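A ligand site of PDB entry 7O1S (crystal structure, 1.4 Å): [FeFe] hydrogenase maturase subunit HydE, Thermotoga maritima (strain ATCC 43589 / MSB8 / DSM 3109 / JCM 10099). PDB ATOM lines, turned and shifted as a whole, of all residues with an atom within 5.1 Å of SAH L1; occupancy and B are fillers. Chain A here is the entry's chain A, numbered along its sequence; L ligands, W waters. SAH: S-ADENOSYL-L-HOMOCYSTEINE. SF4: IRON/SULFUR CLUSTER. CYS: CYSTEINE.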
ATOM      1  N   TYR A  69      10.787 -14.341 -22.295  1.00  0.00           N
ATOM      2  CA  TYR A  69      10.765 -13.574 -21.057  1.00  0.00           C
ATOM      3  C   TYR A  69      10.735 -14.447 -19.805  1.00  0.00           C
ATOM      4  O   TYR A  69      11.013 -13.939 -18.710  1.00  0.00           O
ATOM      5  CB  TYR A  69       9.542 -12.647 -21.035  1.00  0.00           C
ATOM      6  CG  TYR A  69       8.256 -13.307 -21.515  1.00  0.00           C
ATOM      7  CD1 TYR A  69       7.496 -14.093 -20.658  1.00  0.00           C
ATOM      8  CD2 TYR A  69       7.822 -13.159 -22.825  1.00  0.00           C
ATOM      9  CE1 TYR A  69       6.320 -14.710 -21.086  1.00  0.00           C
ATOM     10  CE2 TYR A  69       6.648 -13.762 -23.271  1.00  0.00           C
ATOM     11  CZ  TYR A  69       5.906 -14.540 -22.394  1.00  0.00           C
ATOM     12  OH  TYR A  69       4.750 -15.148 -22.825  1.00  0.00           O
ATOM     13  N   CYS A  70      10.418 -15.736 -19.920  1.00  0.00           N
ATOM     14  CA  CYS A  70       9.980 -16.536 -18.783  1.00  0.00           C
ATOM     15  C   CYS A  70      11.099 -17.405 -18.228  1.00  0.00           C
ATOM     16  O   CYS A  70      11.735 -18.164 -18.962  1.00  0.00           O
ATOM     17  CB  CYS A  70       8.813 -17.437 -19.174  1.00  0.00           C
ATOM     18  SG  CYS A  70       8.126 -18.311 -17.765  1.00  0.00           S
ATOM     19  N   GLY A  71      11.288 -17.329 -16.902  1.00  0.00           N
ATOM     20  CA  GLY A  71      12.281 -18.162 -16.245  1.00  0.00           C
ATOM     21  C   GLY A  71      12.004 -19.656 -16.314  1.00  0.00           C
ATOM     22  O   GLY A  71      12.924 -20.440 -16.102  1.00  0.00           O
ATOM     23  N   GLN A 107      -2.036 -23.201 -11.331  1.00  0.00           N
ATOM     24  CA  GLN A 107      -1.213 -22.652 -12.400  1.00  0.00           C
ATOM     25  C   GLN A 107       0.072 -23.460 -12.538  1.00  0.00           C
ATOM     26  O   GLN A 107       0.613 -23.956 -11.548  1.00  0.00           O
ATOM     27  CB  GLN A 107      -0.848 -21.177 -12.154  1.00  0.00           C
ATOM     28  CG  GLN A 107      -0.155 -20.525 -13.326  1.00  0.00           C
ATOM     29  CD  GLN A 107       0.187 -19.082 -13.096  1.00  0.00           C
ATOM     30  OE1 GLN A 107       1.185 -18.762 -12.441  1.00  0.00           O
ATOM     31  NE2 GLN A 107      -0.636 -18.201 -13.629  1.00  0.00           N
ATOM     32  N   SER A 108       0.561 -23.567 -13.765  1.00  0.00           N
ATOM     33  CA  SER A 108       1.782 -24.333 -14.002  1.00  0.00           C
ATOM     34  C   SER A 108       2.413 -23.895 -15.312  1.00  0.00           C
ATOM     35  O   SER A 108       1.799 -23.189 -16.118  1.00  0.00           O
ATOM     36  CB  SER A 108       1.481 -25.832 -14.077  1.00  0.00           C
ATOM     37  OG  SER A 108       0.594 -26.099 -15.138  1.00  0.00           O
ATOM     38  N   GLY A 109       3.646 -24.349 -15.516  1.00  0.00           N
ATOM     39  CA  GLY A 109       4.183 -24.405 -16.858  1.00  0.00           C
ATOM     40  C   GLY A 109       3.334 -25.343 -17.711  1.00  0.00           C
ATOM     41  O   GLY A 109       2.473 -26.078 -17.225  1.00  0.00           O
ATOM     42  N   GLU A 110       3.561 -25.297 -19.019  1.00  0.00           N
ATOM     43  CA  GLU A 110       2.861 -26.216 -19.917  1.00  0.00           C
ATOM     44  C   GLU A 110       3.524 -27.587 -19.781  1.00  0.00           C
ATOM     45  O   GLU A 110       4.388 -27.978 -20.564  1.00  0.00           O
ATOM     46  CB  GLU A 110       2.888 -25.728 -21.351  1.00  0.00           C
ATOM     47  CG  GLU A 110       1.981 -24.520 -21.567  1.00  0.00           C
ATOM     48  CD  GLU A 110       1.697 -24.274 -23.036  1.00  0.00           C
ATOM     49  OE1 GLU A 110       2.111 -25.104 -23.877  1.00  0.00           O
ATOM     50  OE2 GLU A 110       1.059 -23.245 -23.368  1.00  0.00           O
ATOM     51  N   SER A 136      -4.911 -22.218 -14.977  1.00  0.00           N
ATOM     52  CA  SER A 136      -3.988 -21.338 -15.690  1.00  0.00           C
ATOM     53  C   SER A 136      -2.842 -22.227 -16.149  1.00  0.00           C
ATOM     54  O   SER A 136      -1.752 -22.228 -15.580  1.00  0.00           O
ATOM     55  CB  SER A 136      -3.545 -20.183 -14.791  1.00  0.00           C
ATOM     56  OG  SER A 136      -2.730 -19.248 -15.477  1.00  0.00           O
ATOM     57  N   LEU A 137      -3.094 -23.007 -17.218  1.00  0.00           N
ATOM     58  CA  LEU A 137      -2.192 -24.072 -17.641  1.00  0.00           C
ATOM     59  C   LEU A 137      -1.605 -23.858 -19.019  1.00  0.00           C
ATOM     60  O   LEU A 137      -0.846 -24.718 -19.494  1.00  0.00           O
ATOM     61  CB  LEU A 137      -2.921 -25.421 -17.610  1.00  0.00           C
ATOM     62  CG  LEU A 137      -3.731 -25.732 -16.349  1.00  0.00           C
ATOM     63  CD1 LEU A 137      -4.390 -27.101 -16.465  1.00  0.00           C
ATOM     64  CD2 LEU A 137      -2.850 -25.657 -15.091  1.00  0.00           C
ATOM     65  N   GLY A 138      -1.941 -22.756 -19.682  1.00  0.00           N
ATOM     66  CA  GLY A 138      -1.421 -22.486 -21.011  1.00  0.00           C
ATOM     67  C   GLY A 138      -2.350 -22.941 -22.118  1.00  0.00           C
ATOM     68  O   GLY A 138      -3.575 -23.089 -21.957  1.00  0.00           O
ATOM     69  N   LEU A 157      -7.443 -18.622 -16.795  1.00  0.00           N
ATOM     70  CA  LEU A 157      -6.637 -17.423 -16.967  1.00  0.00           C
ATOM     71  C   LEU A 157      -5.577 -17.719 -18.022  1.00  0.00           C
ATOM     72  O   LEU A 157      -4.708 -18.578 -17.812  1.00  0.00           O
ATOM     73  CB  LEU A 157      -5.995 -17.015 -15.644  1.00  0.00           C
ATOM     74  CG  LEU A 157      -5.033 -15.836 -15.690  1.00  0.00           C
ATOM     75  CD1 LEU A 157      -5.726 -14.552 -16.146  1.00  0.00           C
ATOM     76  CD2 LEU A 157      -4.372 -15.641 -14.318  1.00  0.00           C
ATOM     77  N   LEU A 158      -5.670 -17.044 -19.169  1.00  0.00           N
ATOM     78  CA  LEU A 158      -4.717 -17.196 -20.274  1.00  0.00           C
ATOM     79  C   LEU A 158      -4.353 -15.790 -20.744  1.00  0.00           C
ATOM     80  O   LEU A 158      -4.926 -15.267 -21.705  1.00  0.00           O
ATOM     81  CB  LEU A 158      -5.337 -18.028 -21.383  1.00  0.00           C
ATOM     82  CG  LEU A 158      -4.384 -18.424 -22.500  1.00  0.00           C
ATOM     83  CD1 LEU A 158      -3.415 -19.487 -22.018  1.00  0.00           C
ATOM     84  CD2 LEU A 158      -5.140 -18.916 -23.722  1.00  0.00           C
ATOM     85  N   ARG A 159      -3.396 -15.176 -20.071  1.00  0.00           N
ATOM     86  CA  ARG A 159      -3.064 -13.787 -20.373  1.00  0.00           C
ATOM     87  C   ARG A 159      -2.580 -13.690 -21.810  1.00  0.00           C
ATOM     88  O   ARG A 159      -1.808 -14.539 -22.251  1.00  0.00           O
ATOM     89  CB  ARG A 159      -2.013 -13.294 -19.385  1.00  0.00           C
ATOM     90  CG  ARG A 159      -2.544 -13.212 -17.947  1.00  0.00           C
ATOM     91  CD  ARG A 159      -1.447 -12.944 -16.921  1.00  0.00           C
ATOM     92  NE  ARG A 159      -0.874 -11.605 -17.033  1.00  0.00           N
ATOM     93  CZ  ARG A 159       0.169 -11.167 -16.348  1.00  0.00           C
ATOM     94  NH1 ARG A 159       0.779 -11.946 -15.467  1.00  0.00           N
ATOM     95  NH2 ARG A 159       0.614  -9.933 -16.550  1.00  0.00           N
ATOM     96  N   GLU A 161      -0.672 -11.596 -23.200  1.00  0.00           N
ATOM     97  CA  GLU A 161       0.730 -11.166 -23.197  1.00  0.00           C
ATOM     98  C   GLU A 161       0.969  -9.906 -24.015  1.00  0.00           C
ATOM     99  O   GLU A 161       1.431  -8.893 -23.468  1.00  0.00           O
ATOM    100  CB  GLU A 161       1.690 -12.282 -23.643  1.00  0.00           C
ATOM    101  CG  GLU A 161       1.333 -13.675 -23.104  1.00  0.00           C
ATOM    102  CD  GLU A 161       1.370 -13.809 -21.582  1.00  0.00           C
ATOM    103  OE1 GLU A 161       1.544 -12.812 -20.841  1.00  0.00           O
ATOM    104  OE2 GLU A 161       1.205 -14.961 -21.119  1.00  0.00           O
ATOM    105  N   ARG A 172       7.383 -15.478 -28.219  1.00  0.00           N
ATOM    106  CA  ARG A 172       6.780 -16.770 -27.906  1.00  0.00           C
ATOM    107  C   ARG A 172       6.923 -17.648 -29.141  1.00  0.00           C
ATOM    108  O   ARG A 172       5.960 -17.896 -29.867  1.00  0.00           O
ATOM    109  CB  ARG A 172       5.322 -16.585 -27.474  1.00  0.00           C
ATOM    110  CG  ARG A 172       5.144 -15.478 -26.411  1.00  0.00           C
ATOM    111  CD  ARG A 172       3.755 -15.475 -25.766  1.00  0.00           C
ATOM    112  NE  ARG A 172       3.524 -16.719 -25.033  1.00  0.00           N
ATOM    113  CZ  ARG A 172       2.590 -17.612 -25.331  1.00  0.00           C
ATOM    114  NH1 ARG A 172       1.738 -17.388 -26.334  1.00  0.00           N
ATOM    115  NH2 ARG A 172       2.500 -18.725 -24.621  1.00  0.00           N
ATOM    116  N   ARG A 180      -3.144 -17.981 -29.496  1.00  0.00           N
ATOM    117  CA  ARG A 180      -3.531 -17.544 -28.156  1.00  0.00           C
ATOM    118  C   ARG A 180      -4.963 -17.036 -28.152  1.00  0.00           C
ATOM    119  O   ARG A 180      -5.763 -17.381 -27.268  1.00  0.00           O
ATOM    120  CB  ARG A 180      -2.595 -16.439 -27.695  1.00  0.00           C
ATOM    121  CG  ARG A 180      -2.630 -16.138 -26.193  1.00  0.00           C
ATOM    122  CD  ARG A 180      -1.759 -17.112 -25.466  1.00  0.00           C
ATOM    123  NE  ARG A 180      -1.516 -16.755 -24.064  1.00  0.00           N
ATOM    124  CZ  ARG A 180      -0.883 -17.563 -23.222  1.00  0.00           C
ATOM    125  NH1 ARG A 180      -0.438 -18.740 -23.648  1.00  0.00           N
ATOM    126  NH2 ARG A 180      -0.696 -17.196 -21.955  1.00  0.00           N
ATOM    127  N   MET A 199       1.504  -8.043 -20.458  1.00  0.00           N
ATOM    128  CA  MET A 199       2.639  -7.473 -19.761  1.00  0.00           C
ATOM    129  C   MET A 199       2.924  -6.093 -20.329  1.00  0.00           C
ATOM    130  O   MET A 199       2.678  -5.818 -21.501  1.00  0.00           O
ATOM    131  CB  MET A 199       3.880  -8.362 -19.905  1.00  0.00           C
ATOM    132  CG  MET A 199       3.865  -9.628 -19.041  1.00  0.00           C
ATOM    133  SD  MET A 199       5.300 -10.675 -19.361  1.00  0.00           S
ATOM    134  CE  MET A 199       4.758 -11.438 -20.883  1.00  0.00           C
ATOM    135  N   PRO A 229       3.905  -5.684 -14.938  1.00  0.00           N
ATOM    136  CA  PRO A 229       5.102  -5.269 -15.686  1.00  0.00           C
ATOM    137  C   PRO A 229       5.906  -6.477 -16.090  1.00  0.00           C
ATOM    138  O   PRO A 229       5.874  -7.525 -15.450  1.00  0.00           O
ATOM    139  CB  PRO A 229       5.878  -4.449 -14.636  1.00  0.00           C
ATOM    140  CG  PRO A 229       5.518  -5.135 -13.336  1.00  0.00           C
ATOM    141  CD  PRO A 229       4.075  -5.553 -13.477  1.00  0.00           C
ATOM    142  N   PHE A 230       6.629  -6.323 -17.198  1.00  0.00           N
ATOM    143  CA  PHE A 230       7.676  -7.271 -17.541  1.00  0.00           C
ATOM    144  C   PHE A 230       8.847  -7.118 -16.565  1.00  0.00           C
ATOM    145  O   PHE A 230       9.294  -6.007 -16.286  1.00  0.00           O
ATOM    146  CB  PHE A 230       8.158  -6.996 -18.968  1.00  0.00           C
ATOM    147  CG  PHE A 230       9.519  -7.556 -19.267  1.00  0.00           C
ATOM    148  CD1 PHE A 230       9.730  -8.928 -19.315  1.00  0.00           C
ATOM    149  CD2 PHE A 230      10.595  -6.704 -19.528  1.00  0.00           C
ATOM    150  CE1 PHE A 230      10.995  -9.430 -19.590  1.00  0.00           C
ATOM    151  CE2 PHE A 230      11.847  -7.221 -19.804  1.00  0.00           C
ATOM    152  CZ  PHE A 230      12.047  -8.584 -19.835  1.00  0.00           C
ATOM    153  N   ILE A 231       9.322  -8.238 -16.034  1.00  0.00           N
ATOM    154  CA  ILE A 231      10.448  -8.256 -15.108  1.00  0.00           C
ATOM    155  C   ILE A 231      11.534  -9.158 -15.698  1.00  0.00           C
ATOM    156  O   ILE A 231      11.328 -10.372 -15.806  1.00  0.00           O
ATOM    157  CB  ILE A 231      10.025  -8.732 -13.704  1.00  0.00           C
ATOM    158  CG1 ILE A 231       8.963  -7.783 -13.116  1.00  0.00           C
ATOM    159  CG2 ILE A 231      11.244  -8.834 -12.790  1.00  0.00           C
ATOM    160  CD1 ILE A 231       8.273  -8.336 -11.886  1.00  0.00           C
ATOM    161  N   PRO A 232      12.694  -8.613 -16.082  1.00  0.00           N
ATOM    162  CA  PRO A 232      13.711  -9.444 -16.748  1.00  0.00           C
ATOM    163  C   PRO A 232      14.266 -10.504 -15.822  1.00  0.00           C
ATOM    164  O   PRO A 232      14.454 -10.278 -14.617  1.00  0.00           O
ATOM    165  CB  PRO A 232      14.799  -8.424 -17.137  1.00  0.00           C
ATOM    166  CG  PRO A 232      14.643  -7.331 -16.140  1.00  0.00           C
ATOM    167  CD  PRO A 232      13.162  -7.228 -15.874  1.00  0.00           C
ATOM    168  N   HIS A 233      14.526 -11.686 -16.386  1.00  0.00           N
ATOM    169  CA  HIS A 233      15.036 -12.820 -15.650  1.00  0.00           C
ATOM    170  C   HIS A 233      16.443 -13.116 -16.131  1.00  0.00           C
ATOM    171  O   HIS A 233      16.666 -13.253 -17.350  1.00  0.00           O
ATOM    172  CB  HIS A 233      14.138 -14.040 -15.878  1.00  0.00           C
ATOM    173  CG  HIS A 233      14.439 -15.204 -14.987  1.00  0.00           C
ATOM    174  ND1 HIS A 233      15.665 -15.836 -14.991  1.00  0.00           N
ATOM    175  CD2 HIS A 233      13.686 -15.853 -14.072  1.00  0.00           C
ATOM    176  CE1 HIS A 233      15.646 -16.828 -14.114  1.00  0.00           C
ATOM    177  NE2 HIS A 233      14.461 -16.853 -13.547  1.00  0.00           N
ATOM    178  N   ALA A 270       3.372  -9.573  -9.808  1.00  0.00           N
ATOM    179  CA  ALA A 270       4.429  -8.786 -10.427  1.00  0.00           C
ATOM    180  C   ALA A 270       4.375  -7.330  -9.985  1.00  0.00           C
ATOM    181  O   ALA A 270       5.428  -6.710  -9.797  1.00  0.00           O
ATOM    182  CB  ALA A 270       4.365  -8.912 -11.959  1.00  0.00           C
ATOM    183  N   TYR A 303       9.352 -21.717  -8.462  1.00  0.00           N
ATOM    184  CA  TYR A 303       8.450 -21.212  -9.493  1.00  0.00           C
ATOM    185  C   TYR A 303       8.891 -19.790  -9.880  1.00  0.00           C
ATOM    186  O   TYR A 303       8.265 -18.794  -9.525  1.00  0.00           O
ATOM    187  CB  TYR A 303       7.010 -21.268  -8.999  1.00  0.00           C
ATOM    188  CG  TYR A 303       5.985 -21.146 -10.102  1.00  0.00           C
ATOM    189  CD1 TYR A 303       5.713 -22.217 -10.953  1.00  0.00           C
ATOM    190  CD2 TYR A 303       5.297 -19.963 -10.299  1.00  0.00           C
ATOM    191  CE1 TYR A 303       4.784 -22.111 -11.967  1.00  0.00           C
ATOM    192  CE2 TYR A 303       4.361 -19.838 -11.305  1.00  0.00           C
ATOM    193  CZ  TYR A 303       4.103 -20.912 -12.127  1.00  0.00           C
ATOM    194  OH  TYR A 303       3.169 -20.776 -13.118  1.00  0.00           O
ATOM    195  N   LEU A 305       9.159 -17.484 -12.403  1.00  0.00           N
ATOM    196  CA  LEU A 305       8.814 -16.760 -13.638  1.00  0.00           C
ATOM    197  C   LEU A 305       9.737 -15.568 -13.845  1.00  0.00           C
ATOM    198  O   LEU A 305      10.218 -15.327 -14.954  1.00  0.00           O
ATOM    199  CB  LEU A 305       7.361 -16.291 -13.588  1.00  0.00           C
ATOM    200  CG  LEU A 305       6.260 -17.323 -13.352  1.00  0.00           C
ATOM    201  CD1 LEU A 305       4.935 -16.598 -13.113  1.00  0.00           C
ATOM    202  CD2 LEU A 305       6.141 -18.296 -14.506  1.00  0.00           C
ATOM    203  N   TYR A 306       9.992 -14.818 -12.776  1.00  0.00           N
ATOM    204  CA  TYR A 306      10.889 -13.667 -12.770  1.00  0.00           C
ATOM    205  C   TYR A 306      11.541 -13.601 -11.398  1.00  0.00           C
ATOM    206  O   TYR A 306      11.016 -14.165 -10.438  1.00  0.00           O
ATOM    207  CB  TYR A 306      10.099 -12.383 -13.046  1.00  0.00           C
ATOM    208  CG  TYR A 306       8.783 -12.294 -12.302  1.00  0.00           C
ATOM    209  CD1 TYR A 306       8.717 -11.835 -10.988  1.00  0.00           C
ATOM    210  CD2 TYR A 306       7.587 -12.668 -12.923  1.00  0.00           C
ATOM    211  CE1 TYR A 306       7.508 -11.754 -10.320  1.00  0.00           C
ATOM    212  CE2 TYR A 306       6.383 -12.589 -12.269  1.00  0.00           C
ATOM    213  CZ  TYR A 306       6.337 -12.148 -10.966  1.00  0.00           C
ATOM    214  OH  TYR A 306       5.132 -12.056 -10.307  1.00  0.00           O
HETATM  215  N   SAH L   1       2.174 -21.490 -18.582  1.00  0.00           N
HETATM  216  CA  SAH L   1       0.965 -20.689 -18.401  1.00  0.00           C
HETATM  217  CB  SAH L   1       0.821 -20.186 -16.962  1.00  0.00           C
HETATM  218  CG  SAH L   1       2.085 -19.795 -16.200  1.00  0.00           C
HETATM  219  SD  SAH L   1       2.992 -18.330 -16.786  1.00  0.00           S
HETATM  220  C   SAH L   1       0.880 -19.548 -19.404  1.00  0.00           C
HETATM  221  O   SAH L   1      -0.203 -18.980 -19.628  1.00  0.00           O
HETATM  222  OXT SAH L   1       1.884 -19.148 -20.017  1.00  0.00           O
HETATM  223  C5' SAH L   1       1.835 -17.146 -16.064  1.00  0.00           C
HETATM  224  C4' SAH L   1       2.167 -15.704 -16.468  1.00  0.00           C
HETATM  225  O4' SAH L   1       3.422 -15.289 -15.981  1.00  0.00           O
HETATM  226  C3' SAH L   1       2.254 -15.454 -17.972  1.00  0.00           C
HETATM  227  O3' SAH L   1       0.982 -15.260 -18.542  1.00  0.00           O
HETATM  228  C2' SAH L   1       3.101 -14.192 -18.066  1.00  0.00           C
HETATM  229  O2' SAH L   1       2.299 -13.041 -18.265  1.00  0.00           O
HETATM  230  C1' SAH L   1       3.760 -14.105 -16.688  1.00  0.00           C
HETATM  231  N9  SAH L   1       5.228 -13.937 -16.831  1.00  0.00           N
HETATM  232  C8  SAH L   1       6.117 -14.843 -17.358  1.00  0.00           C
HETATM  233  N7  SAH L   1       7.359 -14.309 -17.339  1.00  0.00           N
HETATM  234  C5  SAH L   1       7.276 -13.051 -16.829  1.00  0.00           C
HETATM  235  C6  SAH L   1       8.232 -12.063 -16.580  1.00  0.00           C
HETATM  236  N6  SAH L   1       9.534 -12.244 -16.869  1.00  0.00           N
HETATM  237  N1  SAH L   1       7.818 -10.859 -16.043  1.00  0.00           N
HETATM  238  C2  SAH L   1       6.491 -10.645 -15.724  1.00  0.00           C
HETATM  239  N3  SAH L   1       5.543 -11.628 -15.963  1.00  0.00           N
HETATM  240  C4  SAH L   1       5.934 -12.812 -16.497  1.00  0.00           C
HETATM  241 FE1  SF4 L   2       6.623 -19.463 -19.011  1.00  0.00          FE
HETATM  242 FE2  SF4 L   2       5.993 -21.847 -20.161  1.00  0.00          FE
HETATM  243 FE3  SF4 L   2       5.773 -19.515 -21.586  1.00  0.00          FE
HETATM  244 FE4  SF4 L   2       3.924 -20.038 -19.502  1.00  0.00          FE
HETATM  245  S1  SF4 L   2       4.229 -21.201 -21.476  1.00  0.00           S
HETATM  246  S2  SF4 L   2       5.056 -18.075 -19.937  1.00  0.00           S
HETATM  247  S3  SF4 L   2       5.374 -21.130 -18.075  1.00  0.00           S
HETATM  248  S4  SF4 L   2       7.716 -20.458 -20.789  1.00  0.00           S
HETATM  249  N   CYS L   3       0.751 -14.584 -10.583  1.00  0.00           N
HETATM  250  CA  CYS L   3       1.879 -14.218 -11.429  1.00  0.00           C
HETATM  251  C   CYS L   3       1.777 -12.726 -11.641  1.00  0.00           C
HETATM  252  O   CYS L   3       0.647 -12.240 -11.728  1.00  0.00           O
HETATM  253  CB  CYS L   3       1.781 -14.917 -12.774  1.00  0.00           C
HETATM  254  SG  CYS L   3       0.134 -14.690 -13.494  1.00  0.00           S
HETATM  255  OXT CYS L   3       2.776 -12.012 -11.733  1.00  0.00           O
HETATM  256  O   HOH W   1      -1.344 -16.682 -18.409  1.00  0.00           O
HETATM  257  O   HOH W   2       1.146 -20.648 -22.476  1.00  0.00           O
HETATM  258  O   HOH W   3       2.830 -16.940 -21.970  1.00  0.00           O
HETATM  259  O   HOH W   4      -2.597 -20.122 -18.639  1.00  0.00           O
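The side-chain hydroxyl (OH) of Tyr 306 is in hydrogen-bond range of the backbone NH (N) of Ala 270, 3.1 Å away. The backbone NH (N) of Ser 108 lies within hydrogen-bond range of the backbone carbonyl oxygen (O) of Ser 136 (3.2 Å). The guanidinium group (NE) of Arg 180 sits at hydrogen-bond distance from the backbone carbonyl oxygen (O) of Arg 159. The backbone carbonyl oxygen (O) of Leu 305 is in hydrogen-bond range of the backbone NH (N) of Gly 71. The side-chain carboxylate of Glu 161 lies within salt-bridge range of the guanidinium group of Arg 180. The side-chain hydroxyl (OH) of Tyr 303 sits at hydrogen-bond distance from the side-chain amide oxygen (OE1) of Gln 107 (2.9 Å). The guanidinium group (NE) of Arg 172 lies within hydrogen-bond range of the side-chain hydroxyl (OH) of Tyr 69. The backbone carbonyl oxygen of Leu 157 sits at hydrogen-bond distance from the side-chain hydroxyl of Ser 136 (3.1 Å).
The guanidinium group (NH1) of Arg 159 sits close to a sulfur (SG) of CYS L3 (3.4 Å). N6 of SAH L1 is in hydrogen-bond range of O of Tyr 69, at 2.9 Å. The backbone NH of Ala 270 lies within hydrogen-bond range of an oxygen (OXT) of CYS L3 (3.2 Å). NE2 of Gln 107 lies close to SG of CYS L3. OH of Tyr 306 lies within hydrogen-bond range of OXT of CYS L3. A nitrogen (N) of SAH L1 lies close to the backbone carbonyl oxygen of Ser 108 (3.0 Å). The backbone NH (N) of Ile 231 is in hydrogen-bond range of a nitrogen (N1) of SAH L1, at 3.0 Å. N6 of SAH L1 lies within hydrogen-bond range of O of Ile 231 (2.8 Å). FE1 of SF4 L2 is bound by SG of Cys 70, 2.3 Å away. The guanidinium group of Arg 180 lies within salt-bridge range of an oxygen (O) of SAH L1, at 3.0 Å. An oxygen (O2') of SAH L1 lies within hydrogen-bond range of the guanidinium group (NH1) of Arg 159 (3.4 Å). An oxygen (O3') of SAH L1 lies within hydrogen-bond range of the side-chain carboxylate of Glu 161, 2.6 Å away.
N3 of SAH L1 lies close to SD of Met 199 (3.5 Å). Residues that only touch SAH L1: Cys 70 (3.7 Å), Gln 107 (3.6 Å), Gly 109 (3.9 Å), Ser 136 (3.6 Å), Gly 138 (3.8 Å), Pro 229 (3.2 Å), Phe 230 (3.9 Å), Tyr 303 (3.4 Å), Leu 305 (3.5 Å) and Tyr 306 (3.6 Å). Hydrophobic or aromatic side chains within 4 Å of SAH L1: Tyr 69, Met 199, Ile 231, Leu 305 and Tyr 306. 17 residues have an atom within 4 Å of SAH L1: Tyr 69, Cys 70, Gln 107, Ser 108, Gly 109, Ser 136, Gly 138, Arg 159, Glu 161, Arg 180, Met 199, Pro 229, Phe 230, Ile 231, Tyr 303, Leu 305 and Tyr 306. The nearest printed residue that does not touch SAH L1 is Leu 158 (4.04 Å).
FE4 of SF4 L2 is bound by OXT of SAH L1, at 2.3 Å.
Water W1 lies within hydrogen-bond range of O3' of SAH L1 (2.7 Å) and N of Arg 159 (3.0 Å). Water W4 lies within hydrogen-bond range of the backbone carbonyl oxygen of Leu 157 (2.7 Å), an oxygen (O) of SAH L1 (2.8 Å), the backbone NH of Gly 138 (2.9 Å), the backbone NH of Leu 137 (3.3 Å) and the side-chain hydroxyl of Ser 136 (3.3 Å). Water W2 lies within hydrogen-bond range of NH1 of Arg 180, OE2 of Glu 110, NH2 of Arg 172 and S1 of SF4 L2. Water W3 lies within hydrogen-bond range of OE2 of Glu 161, OH of Tyr 69, NE of Arg 172 and S2 of SF4 L2.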
